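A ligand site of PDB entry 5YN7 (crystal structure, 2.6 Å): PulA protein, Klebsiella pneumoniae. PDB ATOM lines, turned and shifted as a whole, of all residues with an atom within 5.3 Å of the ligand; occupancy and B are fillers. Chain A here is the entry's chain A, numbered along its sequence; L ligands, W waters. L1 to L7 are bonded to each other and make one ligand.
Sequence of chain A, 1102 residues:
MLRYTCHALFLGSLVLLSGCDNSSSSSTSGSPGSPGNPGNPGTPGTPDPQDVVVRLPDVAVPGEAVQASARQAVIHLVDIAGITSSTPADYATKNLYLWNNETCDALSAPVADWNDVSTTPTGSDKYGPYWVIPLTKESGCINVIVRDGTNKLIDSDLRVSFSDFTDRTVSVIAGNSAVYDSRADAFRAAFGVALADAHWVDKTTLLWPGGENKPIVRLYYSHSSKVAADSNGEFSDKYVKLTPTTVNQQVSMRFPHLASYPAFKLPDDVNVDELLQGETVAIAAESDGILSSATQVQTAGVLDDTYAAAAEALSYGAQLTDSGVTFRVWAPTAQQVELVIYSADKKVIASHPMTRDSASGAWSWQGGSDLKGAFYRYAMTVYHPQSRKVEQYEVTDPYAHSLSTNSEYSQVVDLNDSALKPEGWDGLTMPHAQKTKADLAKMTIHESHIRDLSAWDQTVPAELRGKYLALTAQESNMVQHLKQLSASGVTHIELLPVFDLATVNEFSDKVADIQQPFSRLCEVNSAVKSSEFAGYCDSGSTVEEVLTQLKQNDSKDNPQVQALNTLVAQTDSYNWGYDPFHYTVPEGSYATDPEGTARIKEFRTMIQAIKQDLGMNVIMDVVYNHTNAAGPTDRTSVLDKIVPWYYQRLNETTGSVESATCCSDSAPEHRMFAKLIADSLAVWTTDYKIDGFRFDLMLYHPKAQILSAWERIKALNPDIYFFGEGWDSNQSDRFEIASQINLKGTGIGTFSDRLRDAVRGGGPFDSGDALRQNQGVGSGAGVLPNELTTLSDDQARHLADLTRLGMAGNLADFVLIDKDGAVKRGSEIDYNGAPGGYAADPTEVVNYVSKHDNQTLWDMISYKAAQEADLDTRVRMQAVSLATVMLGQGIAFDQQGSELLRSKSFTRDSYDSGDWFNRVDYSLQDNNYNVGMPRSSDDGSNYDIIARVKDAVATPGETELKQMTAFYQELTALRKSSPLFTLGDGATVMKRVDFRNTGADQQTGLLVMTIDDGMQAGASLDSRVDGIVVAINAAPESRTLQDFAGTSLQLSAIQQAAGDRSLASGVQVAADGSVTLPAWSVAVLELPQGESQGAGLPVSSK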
ATOM      1  N   TRP A 727     -18.240  -7.085 -14.887  1.00  0.00           N
ATOM      2  CA  TRP A 727     -16.885  -7.249 -15.404  1.00  0.00           C
ATOM      3  C   TRP A 727     -16.415  -6.163 -16.364  1.00  0.00           C
ATOM      4  O   TRP A 727     -15.209  -5.930 -16.450  1.00  0.00           O
ATOM      5  CB  TRP A 727     -16.755  -8.582 -16.126  1.00  0.00           C
ATOM      6  CG  TRP A 727     -17.939  -9.485 -15.941  1.00  0.00           C
ATOM      7  CD1 TRP A 727     -19.162  -9.396 -16.574  1.00  0.00           C
ATOM      8  CD2 TRP A 727     -18.005 -10.637 -15.098  1.00  0.00           C
ATOM      9  NE1 TRP A 727     -19.979 -10.426 -16.154  1.00  0.00           N
ATOM     10  CE2 TRP A 727     -19.283 -11.202 -15.254  1.00  0.00           C
ATOM     11  CE3 TRP A 727     -17.105 -11.261 -14.218  1.00  0.00           C
ATOM     12  CZ2 TRP A 727     -19.671 -12.363 -14.573  1.00  0.00           C
ATOM     13  CZ3 TRP A 727     -17.514 -12.396 -13.535  1.00  0.00           C
ATOM     14  CH2 TRP A 727     -18.787 -12.936 -13.707  1.00  0.00           C
ATOM     15  N   ASP A 728     -17.304  -5.496 -17.098  1.00  0.00           N
ATOM     16  CA  ASP A 728     -16.863  -4.529 -18.103  1.00  0.00           C
ATOM     17  C   ASP A 728     -17.075  -3.095 -17.624  1.00  0.00           C
ATOM     18  O   ASP A 728     -16.107  -2.360 -17.388  1.00  0.00           O
ATOM     19  CB  ASP A 728     -17.593  -4.759 -19.424  1.00  0.00           C
ATOM     20  CG  ASP A 728     -18.696  -5.810 -19.331  1.00  0.00           C
ATOM     21  OD1 ASP A 728     -19.004  -6.267 -18.200  1.00  0.00           O
ATOM     22  OD2 ASP A 728     -19.254  -6.191 -20.383  1.00  0.00           O
ATOM     23  N   ASP A 753     -15.130 -14.592 -10.830  1.00  0.00           N
ATOM     24  CA  ASP A 753     -14.808 -15.382 -12.002  1.00  0.00           C
ATOM     25  C   ASP A 753     -13.495 -16.132 -11.857  1.00  0.00           C
ATOM     26  O   ASP A 753     -13.119 -16.861 -12.782  1.00  0.00           O
ATOM     27  CB  ASP A 753     -14.792 -14.502 -13.257  1.00  0.00           C
ATOM     28  CG  ASP A 753     -14.272 -13.114 -12.990  1.00  0.00           C
ATOM     29  OD1 ASP A 753     -13.997 -12.760 -11.819  1.00  0.00           O
ATOM     30  OD2 ASP A 753     -14.070 -12.381 -13.990  1.00  0.00           O
ATOM     31  N   ARG A 756     -14.060 -19.980 -10.847  1.00  0.00           N
ATOM     32  CA  ARG A 756     -14.822 -20.375 -12.022  1.00  0.00           C
ATOM     33  C   ARG A 756     -13.924 -20.714 -13.204  1.00  0.00           C
ATOM     34  O   ARG A 756     -13.961 -21.825 -13.740  1.00  0.00           O
ATOM     35  CB  ARG A 756     -15.790 -19.262 -12.399  1.00  0.00           C
ATOM     36  CG  ARG A 756     -16.860 -19.670 -13.417  1.00  0.00           C
ATOM     37  CD  ARG A 756     -17.320 -18.502 -14.283  1.00  0.00           C
ATOM     38  NE  ARG A 756     -16.217 -17.698 -14.820  1.00  0.00           N
ATOM     39  CZ  ARG A 756     -16.387 -16.571 -15.512  1.00  0.00           C
ATOM     40  NH1 ARG A 756     -17.591 -16.083 -15.739  1.00  0.00           N
ATOM     41  NH2 ARG A 756     -15.331 -15.914 -15.980  1.00  0.00           N
ATOM     42  N   ASP A 757     -13.112 -19.749 -13.631  1.00  0.00           N
ATOM     43  CA  ASP A 757     -12.241 -20.005 -14.772  1.00  0.00           C
ATOM     44  C   ASP A 757     -11.189 -21.070 -14.443  1.00  0.00           C
ATOM     45  O   ASP A 757     -10.702 -21.774 -15.342  1.00  0.00           O
ATOM     46  CB  ASP A 757     -11.584 -18.702 -15.222  1.00  0.00           C
ATOM     47  CG  ASP A 757     -12.560 -17.757 -15.959  1.00  0.00           C
ATOM     48  OD1 ASP A 757     -13.716 -18.141 -16.244  1.00  0.00           O
ATOM     49  OD2 ASP A 757     -12.150 -16.615 -16.278  1.00  0.00           O
ATOM     50  N   GLY A 763     -11.959 -19.312 -20.543  1.00  0.00           N
ATOM     51  CA  GLY A 763     -12.755 -18.154 -20.250  1.00  0.00           C
ATOM     52  C   GLY A 763     -13.937 -18.048 -21.187  1.00  0.00           C
ATOM     53  O   GLY A 763     -14.159 -18.889 -22.070  1.00  0.00           O
ATOM     54  N   PRO A 764     -14.732 -16.988 -21.002  1.00  0.00           N
ATOM     55  CA  PRO A 764     -16.006 -16.874 -21.745  1.00  0.00           C
ATOM     56  C   PRO A 764     -15.843 -16.574 -23.234  1.00  0.00           C
ATOM     57  O   PRO A 764     -16.765 -16.880 -24.003  1.00  0.00           O
ATOM     58  CB  PRO A 764     -16.733 -15.727 -21.015  1.00  0.00           C
ATOM     59  CG  PRO A 764     -15.950 -15.490 -19.740  1.00  0.00           C
ATOM     60  CD  PRO A 764     -14.543 -15.899 -20.026  1.00  0.00           C
ATOM     61  N   PHE A 765     -14.702 -16.015 -23.650  1.00  0.00           N
ATOM     62  CA  PHE A 765     -14.484 -15.644 -25.040  1.00  0.00           C
ATOM     63  C   PHE A 765     -14.029 -16.804 -25.914  1.00  0.00           C
ATOM     64  O   PHE A 765     -14.083 -16.681 -27.138  1.00  0.00           O
ATOM     65  CB  PHE A 765     -13.444 -14.527 -25.146  1.00  0.00           C
ATOM     66  CG  PHE A 765     -13.713 -13.334 -24.245  1.00  0.00           C
ATOM     67  CD1 PHE A 765     -12.681 -12.772 -23.497  1.00  0.00           C
ATOM     68  CD2 PHE A 765     -14.980 -12.757 -24.172  1.00  0.00           C
ATOM     69  CE1 PHE A 765     -12.910 -11.684 -22.672  1.00  0.00           C
ATOM     70  CE2 PHE A 765     -15.210 -11.669 -23.346  1.00  0.00           C
ATOM     71  CZ  PHE A 765     -14.176 -11.130 -22.590  1.00  0.00           C
ATOM     72  N   ASP A 766     -13.596 -17.920 -25.309  1.00  0.00           N
ATOM     73  CA  ASP A 766     -13.013 -19.035 -26.039  1.00  0.00           C
ATOM     74  C   ASP A 766     -13.964 -19.533 -27.124  1.00  0.00           C
ATOM     75  O   ASP A 766     -15.182 -19.558 -26.950  1.00  0.00           O
ATOM     76  CB  ASP A 766     -12.723 -20.195 -25.092  1.00  0.00           C
ATOM     77  CG  ASP A 766     -11.717 -19.837 -24.036  1.00  0.00           C
ATOM     78  OD1 ASP A 766     -11.300 -18.669 -23.966  1.00  0.00           O
ATOM     79  OD2 ASP A 766     -11.369 -20.742 -23.242  1.00  0.00           O
ATOM     80  N   SER A 767     -13.383 -19.968 -28.236  1.00  0.00           N
ATOM     81  CA  SER A 767     -14.145 -20.659 -29.270  1.00  0.00           C
ATOM     82  C   SER A 767     -13.190 -21.550 -30.024  1.00  0.00           C
ATOM     83  O   SER A 767     -11.971 -21.468 -29.876  1.00  0.00           O
ATOM     84  CB  SER A 767     -14.842 -19.686 -30.228  1.00  0.00           C
ATOM     85  OG  SER A 767     -13.906 -18.880 -30.918  1.00  0.00           O
ATOM     86  N   TYR A 831      -4.939 -12.651 -11.799  1.00  0.00           N
ATOM     87  CA  TYR A 831      -6.084 -13.123 -12.570  1.00  0.00           C
ATOM     88  C   TYR A 831      -6.163 -12.209 -13.793  1.00  0.00           C
ATOM     89  O   TYR A 831      -6.785 -11.148 -13.754  1.00  0.00           O
ATOM     90  CB  TYR A 831      -7.365 -13.107 -11.749  1.00  0.00           C
ATOM     91  CG  TYR A 831      -8.595 -13.530 -12.530  1.00  0.00           C
ATOM     92  CD1 TYR A 831      -8.720 -14.827 -13.005  1.00  0.00           C
ATOM     93  CD2 TYR A 831      -9.626 -12.629 -12.802  1.00  0.00           C
ATOM     94  CE1 TYR A 831      -9.834 -15.225 -13.713  1.00  0.00           C
ATOM     95  CE2 TYR A 831     -10.752 -13.013 -13.517  1.00  0.00           C
ATOM     96  CZ  TYR A 831     -10.850 -14.318 -13.969  1.00  0.00           C
ATOM     97  OH  TYR A 831     -11.952 -14.730 -14.670  1.00  0.00           O
ATOM     98  N   ASN A 832      -5.521 -12.648 -14.877  1.00  0.00           N
ATOM     99  CA  ASN A 832      -5.500 -11.920 -16.129  1.00  0.00           C
ATOM    100  C   ASN A 832      -5.063 -10.470 -15.908  1.00  0.00           C
ATOM    101  O   ASN A 832      -5.713  -9.533 -16.332  1.00  0.00           O
ATOM    102  CB  ASN A 832      -6.867 -12.000 -16.817  1.00  0.00           C
ATOM    103  CG  ASN A 832      -7.312 -13.428 -17.040  1.00  0.00           C
ATOM    104  OD1 ASN A 832      -6.500 -14.264 -17.397  1.00  0.00           O
ATOM    105  ND2 ASN A 832      -8.584 -13.719 -16.822  1.00  0.00           N
ATOM    106  N   ASP A 853     -25.774 -18.346 -17.893  1.00  0.00           N
ATOM    107  CA  ASP A 853     -25.101 -17.875 -19.087  1.00  0.00           C
ATOM    108  C   ASP A 853     -23.784 -18.632 -19.260  1.00  0.00           C
ATOM    109  O   ASP A 853     -23.189 -19.100 -18.286  1.00  0.00           O
ATOM    110  CB  ASP A 853     -24.866 -16.354 -19.073  1.00  0.00           C
ATOM    111  CG  ASP A 853     -24.098 -15.867 -17.840  1.00  0.00           C
ATOM    112  OD1 ASP A 853     -24.187 -16.490 -16.761  1.00  0.00           O
ATOM    113  OD2 ASP A 853     -23.415 -14.817 -17.946  1.00  0.00           O
ATOM    114  N   ASN A 854     -23.369 -18.781 -20.530  1.00  0.00           N
ATOM    115  CA  ASN A 854     -22.236 -19.598 -20.974  1.00  0.00           C
ATOM    116  C   ASN A 854     -22.519 -21.100 -20.874  1.00  0.00           C
ATOM    117  O   ASN A 854     -23.589 -21.514 -20.407  1.00  0.00           O
ATOM    118  CB  ASN A 854     -20.985 -19.183 -20.217  1.00  0.00           C
ATOM    119  CG  ASN A 854     -20.603 -17.752 -20.510  1.00  0.00           C
ATOM    120  OD1 ASN A 854     -20.432 -17.401 -21.672  1.00  0.00           O
ATOM    121  ND2 ASN A 854     -20.511 -16.922 -19.487  1.00  0.00           N
ATOM    122  N   ARG A 908     -23.953 -22.200 -25.920  1.00  0.00           N
ATOM    123  CA  ARG A 908     -23.311 -21.316 -24.971  1.00  0.00           C
ATOM    124  C   ARG A 908     -24.241 -20.247 -24.408  1.00  0.00           C
ATOM    125  O   ARG A 908     -24.074 -19.862 -23.244  1.00  0.00           O
ATOM    126  CB  ARG A 908     -22.080 -20.688 -25.619  1.00  0.00           C
ATOM    127  CG  ARG A 908     -21.372 -19.710 -24.708  1.00  0.00           C
ATOM    128  CD  ARG A 908     -21.787 -18.329 -25.056  1.00  0.00           C
ATOM    129  NE  ARG A 908     -21.468 -18.140 -26.445  1.00  0.00           N
ATOM    130  CZ  ARG A 908     -20.464 -17.398 -26.854  1.00  0.00           C
ATOM    131  NH1 ARG A 908     -20.211 -17.269 -28.141  1.00  0.00           N
ATOM    132  NH2 ARG A 908     -19.723 -16.768 -25.954  1.00  0.00           N
ATOM    133  N   ASP A 938     -24.530 -18.085 -32.842  1.00  0.00           N
ATOM    134  CA  ASP A 938     -23.654 -17.895 -31.702  1.00  0.00           C
ATOM    135  C   ASP A 938     -22.618 -18.996 -31.523  1.00  0.00           C
ATOM    136  O   ASP A 938     -21.572 -18.747 -30.932  1.00  0.00           O
ATOM    137  CB  ASP A 938     -24.464 -17.783 -30.420  1.00  0.00           C
ATOM    138  CG  ASP A 938     -23.644 -17.240 -29.275  1.00  0.00           C
ATOM    139  OD1 ASP A 938     -23.075 -16.137 -29.444  1.00  0.00           O
ATOM    140  OD2 ASP A 938     -23.561 -17.900 -28.228  1.00  0.00           O
HETATM  141  C1  LIG L   1     -17.108 -11.152 -18.677  1.00  0.00           C
HETATM  142  C2  LIG L   1     -18.199 -12.225 -18.482  1.00  0.00           C
HETATM  143  C3  LIG L   1     -18.805 -12.667 -19.817  1.00  0.00           C
HETATM  144  C4  LIG L   1     -19.091 -11.475 -20.737  1.00  0.00           C
HETATM  145  C5  LIG L   1     -17.871 -10.582 -20.835  1.00  0.00           C
HETATM  146  C6  LIG L   1     -18.092  -9.397 -21.795  1.00  0.00           C
HETATM  147  O1  LIG L   1     -17.678 -13.291 -17.712  1.00  0.00           O
HETATM  148  O2  LIG L   1     -19.994 -13.411 -19.593  1.00  0.00           O
HETATM  149  O3  LIG L   1     -19.226 -11.912 -22.052  1.00  0.00           O
HETATM  150  O4  LIG L   1     -17.534 -10.129 -19.552  1.00  0.00           O
HETATM  151  O5  LIG L   1     -19.228  -8.661 -21.390  1.00  0.00           O
HETATM  152  C1  LG2 L   2     -20.581 -12.002 -22.481  1.00  0.00           C
HETATM  153  C2  LG2 L   2     -20.623 -13.404 -23.048  1.00  0.00           C
HETATM  154  C3  LG2 L   2     -19.410 -13.463 -23.972  1.00  0.00           C
HETATM  155  C4  LG2 L   2     -19.579 -12.464 -25.129  1.00  0.00           C
HETATM  156  C5  LG2 L   2     -19.846 -11.056 -24.527  1.00  0.00           C
HETATM  157  C6  LG2 L   2     -20.257 -10.021 -25.565  1.00  0.00           C
HETATM  158  O1  LG2 L   2     -20.478 -14.324 -22.001  1.00  0.00           O
HETATM  159  O2  LG2 L   2     -19.157 -14.783 -24.409  1.00  0.00           O
HETATM  160  O3  LG2 L   2     -18.425 -12.490 -25.946  1.00  0.00           O
HETATM  161  O4  LG2 L   2     -20.850 -11.085 -23.518  1.00  0.00           O
HETATM  162  O5  LG2 L   2     -19.101  -9.432 -26.112  1.00  0.00           O
HETATM  163  C1  LG3 L   3     -11.936 -10.929 -18.145  1.00  0.00           C
HETATM  164  C2  LG3 L   3     -12.623 -11.738 -17.059  1.00  0.00           C
HETATM  165  C3  LG3 L   3     -13.974 -12.206 -17.562  1.00  0.00           C
HETATM  166  C4  LG3 L   3     -14.797 -11.060 -18.170  1.00  0.00           C
HETATM  167  C5  LG3 L   3     -13.941 -10.031 -18.956  1.00  0.00           C
HETATM  168  C6  LG3 L   3     -14.604  -8.680 -19.139  1.00  0.00           C
HETATM  169  O1  LG3 L   3     -11.814 -12.834 -16.685  1.00  0.00           O
HETATM  170  O2  LG3 L   3     -14.701 -12.812 -16.511  1.00  0.00           O
HETATM  171  O3  LG3 L   3     -15.769 -11.686 -19.006  1.00  0.00           O
HETATM  172  O4  LG3 L   3     -12.703  -9.765 -18.323  1.00  0.00           O
HETATM  173  O5  LG3 L   3     -15.130  -8.583 -20.445  1.00  0.00           O
HETATM  174  C1  LG4 L   4     -18.763 -12.597 -27.357  1.00  0.00           C
HETATM  175  C2  LG4 L   4     -18.098 -13.784 -28.031  1.00  0.00           C
HETATM  176  C3  LG4 L   4     -16.586 -13.604 -28.126  1.00  0.00           C
HETATM  177  C4  LG4 L   4     -16.198 -12.216 -28.647  1.00  0.00           C
HETATM  178  C5  LG4 L   4     -17.072 -11.109 -28.050  1.00  0.00           C
HETATM  179  C6  LG4 L   4     -16.878  -9.754 -28.747  1.00  0.00           C
HETATM  180  O1  LG4 L   4     -18.396 -14.961 -27.312  1.00  0.00           O
HETATM  181  O2  LG4 L   4     -16.031 -14.631 -28.939  1.00  0.00           O
HETATM  182  O3  LG4 L   4     -14.839 -11.996 -28.303  1.00  0.00           O
HETATM  183  O4  LG4 L   4     -18.442 -11.442 -28.102  1.00  0.00           O
HETATM  184  O5  LG4 L   4     -16.785  -9.918 -30.137  1.00  0.00           O
HETATM  185  C1  LG5 L   5      -8.858 -12.956 -21.892  1.00  0.00           C
HETATM  186  C2  LG5 L   5      -9.492 -14.001 -20.961  1.00  0.00           C
HETATM  187  C3  LG5 L   5     -10.769 -13.482 -20.303  1.00  0.00           C
HETATM  188  C4  LG5 L   5     -10.591 -12.068 -19.747  1.00  0.00           C
HETATM  189  C5  LG5 L   5     -10.003 -11.222 -20.873  1.00  0.00           C
HETATM  190  C6  LG5 L   5      -9.972  -9.719 -20.636  1.00  0.00           C
HETATM  191  O1  LG5 L   5      -9.794 -15.172 -21.690  1.00  0.00           O
HETATM  192  O2  LG5 L   5     -11.261 -14.353 -19.304  1.00  0.00           O
HETATM  193  O3  LG5 L   5     -11.886 -11.631 -19.405  1.00  0.00           O
HETATM  194  O4  LG5 L   5      -8.718 -11.726 -21.215  1.00  0.00           O
HETATM  195  O5  LG5 L   5     -11.199  -9.203 -21.099  1.00  0.00           O
HETATM  196  C1  LG6 L   6     -14.062 -11.710 -29.479  1.00  0.00           C
HETATM  197  C2  LG6 L   6     -13.185 -12.901 -29.860  1.00  0.00           C
HETATM  198  C3  LG6 L   6     -12.263 -13.228 -28.696  1.00  0.00           C
HETATM  199  C4  LG6 L   6     -11.481 -11.983 -28.269  1.00  0.00           C
HETATM  200  C5  LG6 L   6     -12.323 -10.701 -28.205  1.00  0.00           C
HETATM  201  C6  LG6 L   6     -11.456  -9.438 -28.235  1.00  0.00           C
HETATM  202  O1  LG6 L   6     -13.979 -14.022 -30.168  1.00  0.00           O
HETATM  203  O2  LG6 L   6     -11.413 -14.303 -29.057  1.00  0.00           O
HETATM  204  O3  LG6 L   6     -10.944 -12.246 -26.998  1.00  0.00           O
HETATM  205  O4  LG6 L   6     -13.228 -10.587 -29.287  1.00  0.00           O
HETATM  206  O5  LG6 L   6     -10.791  -9.244 -27.012  1.00  0.00           O
HETATM  207  C1  LG7 L   7      -9.499 -12.213 -27.044  1.00  0.00           C
HETATM  208  C2  LG7 L   7      -8.890 -13.536 -26.583  1.00  0.00           C
HETATM  209  C3  LG7 L   7      -9.241 -13.799 -25.119  1.00  0.00           C
HETATM  210  C4  LG7 L   7      -9.043 -12.565 -24.233  1.00  0.00           C
HETATM  211  C5  LG7 L   7      -9.650 -11.348 -24.929  1.00  0.00           C
HETATM  212  C6  LG7 L   7      -9.533 -10.051 -24.142  1.00  0.00           C
HETATM  213  O1  LG7 L   7      -9.319 -14.608 -27.402  1.00  0.00           O
HETATM  214  O2  LG7 L   7      -8.473 -14.858 -24.606  1.00  0.00           O
HETATM  215  O3  LG7 L   7      -9.726 -12.794 -23.024  1.00  0.00           O
HETATM  216  O4  LG7 L   7      -9.047 -11.187 -26.189  1.00  0.00           O
HETATM  217  O5  LG7 L   7      -8.228  -9.930 -23.626  1.00  0.00           O
HETATM  218  O   HOH W   1     -12.020 -15.959 -22.575  1.00  0.00           O
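O of Pro 764 sits at hydrogen-bond distance from O2 of LG2 L2 (3.2 Å).
ND2 of Asn 832 sits at hydrogen-bond distance from O1 of LG3 L3.
OD2 of Asp 728 lies within hydrogen-bond range of O5 of LIG L1.
OH of Tyr 831 sits at hydrogen-bond distance from O1 of LG3 L3 (2.8 Å).
The side-chain carboxylate (OD2) of Asp 753 is in hydrogen-bond range of an oxygen (O2) of LG3 L3 (2.6 Å).
An oxygen (O2) of LG2 L2 sits at hydrogen-bond distance from the guanidinium group of Arg 908, 2.6 Å away.
The guanidinium group of Arg 756 sits at hydrogen-bond distance from an oxygen (O2) of LG3 L3, at 3.2 Å.
O of Phe 765 lies within hydrogen-bond range of O2 of LG4 L4 (3.4 Å).
OD1 of Asn 854 sits at hydrogen-bond distance from O1 of LG2 L2 (3.1 Å).
The side-chain hydroxyl (OH) of Tyr 831 lies within hydrogen-bond range of the side-chain carboxylate (OD2) of Asp 757, 2.5 Å away.
The guanidinium group (NE) of Arg 908 lies within salt-bridge range of the side-chain carboxylate (OD2) of Asp 938 (2.8 Å).
O of Arg 908 lies close to N of Asn 854, at 3.0 Å.
The guanidinium group (NH2) of Arg 756 is in salt-bridge range of the side-chain carboxylate (OD1) of Asp 757, 2.8 Å away.
The side-chain hydroxyl of Tyr 831 is in hydrogen-bond range of the backbone carbonyl oxygen of Asp 753 (3.1 Å).
CG of Trp 727 touches C1 of LIG L1 (3.3 Å).
OD2 of Asp 757 touches O1 of LG3 L3, 3.8 Å away.
Hydrophobic or aromatic side chains that line the ligand: Trp 727, Pro 764, Phe 765 and Tyr 831.
Within 4 Å of the ligand: Trp 727, Asp 728, Asp 753, Arg 756, Asp 757, Pro 764, Phe 765, Tyr 831, Asn 832, Asn 854 and Arg 908.
Water W1 lies within hydrogen-bond range of O1 of LG5 L5 (2.5 Å), N of Phe 765 (2.9 Å) and OD1 of Asp 766 (3.1 Å).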
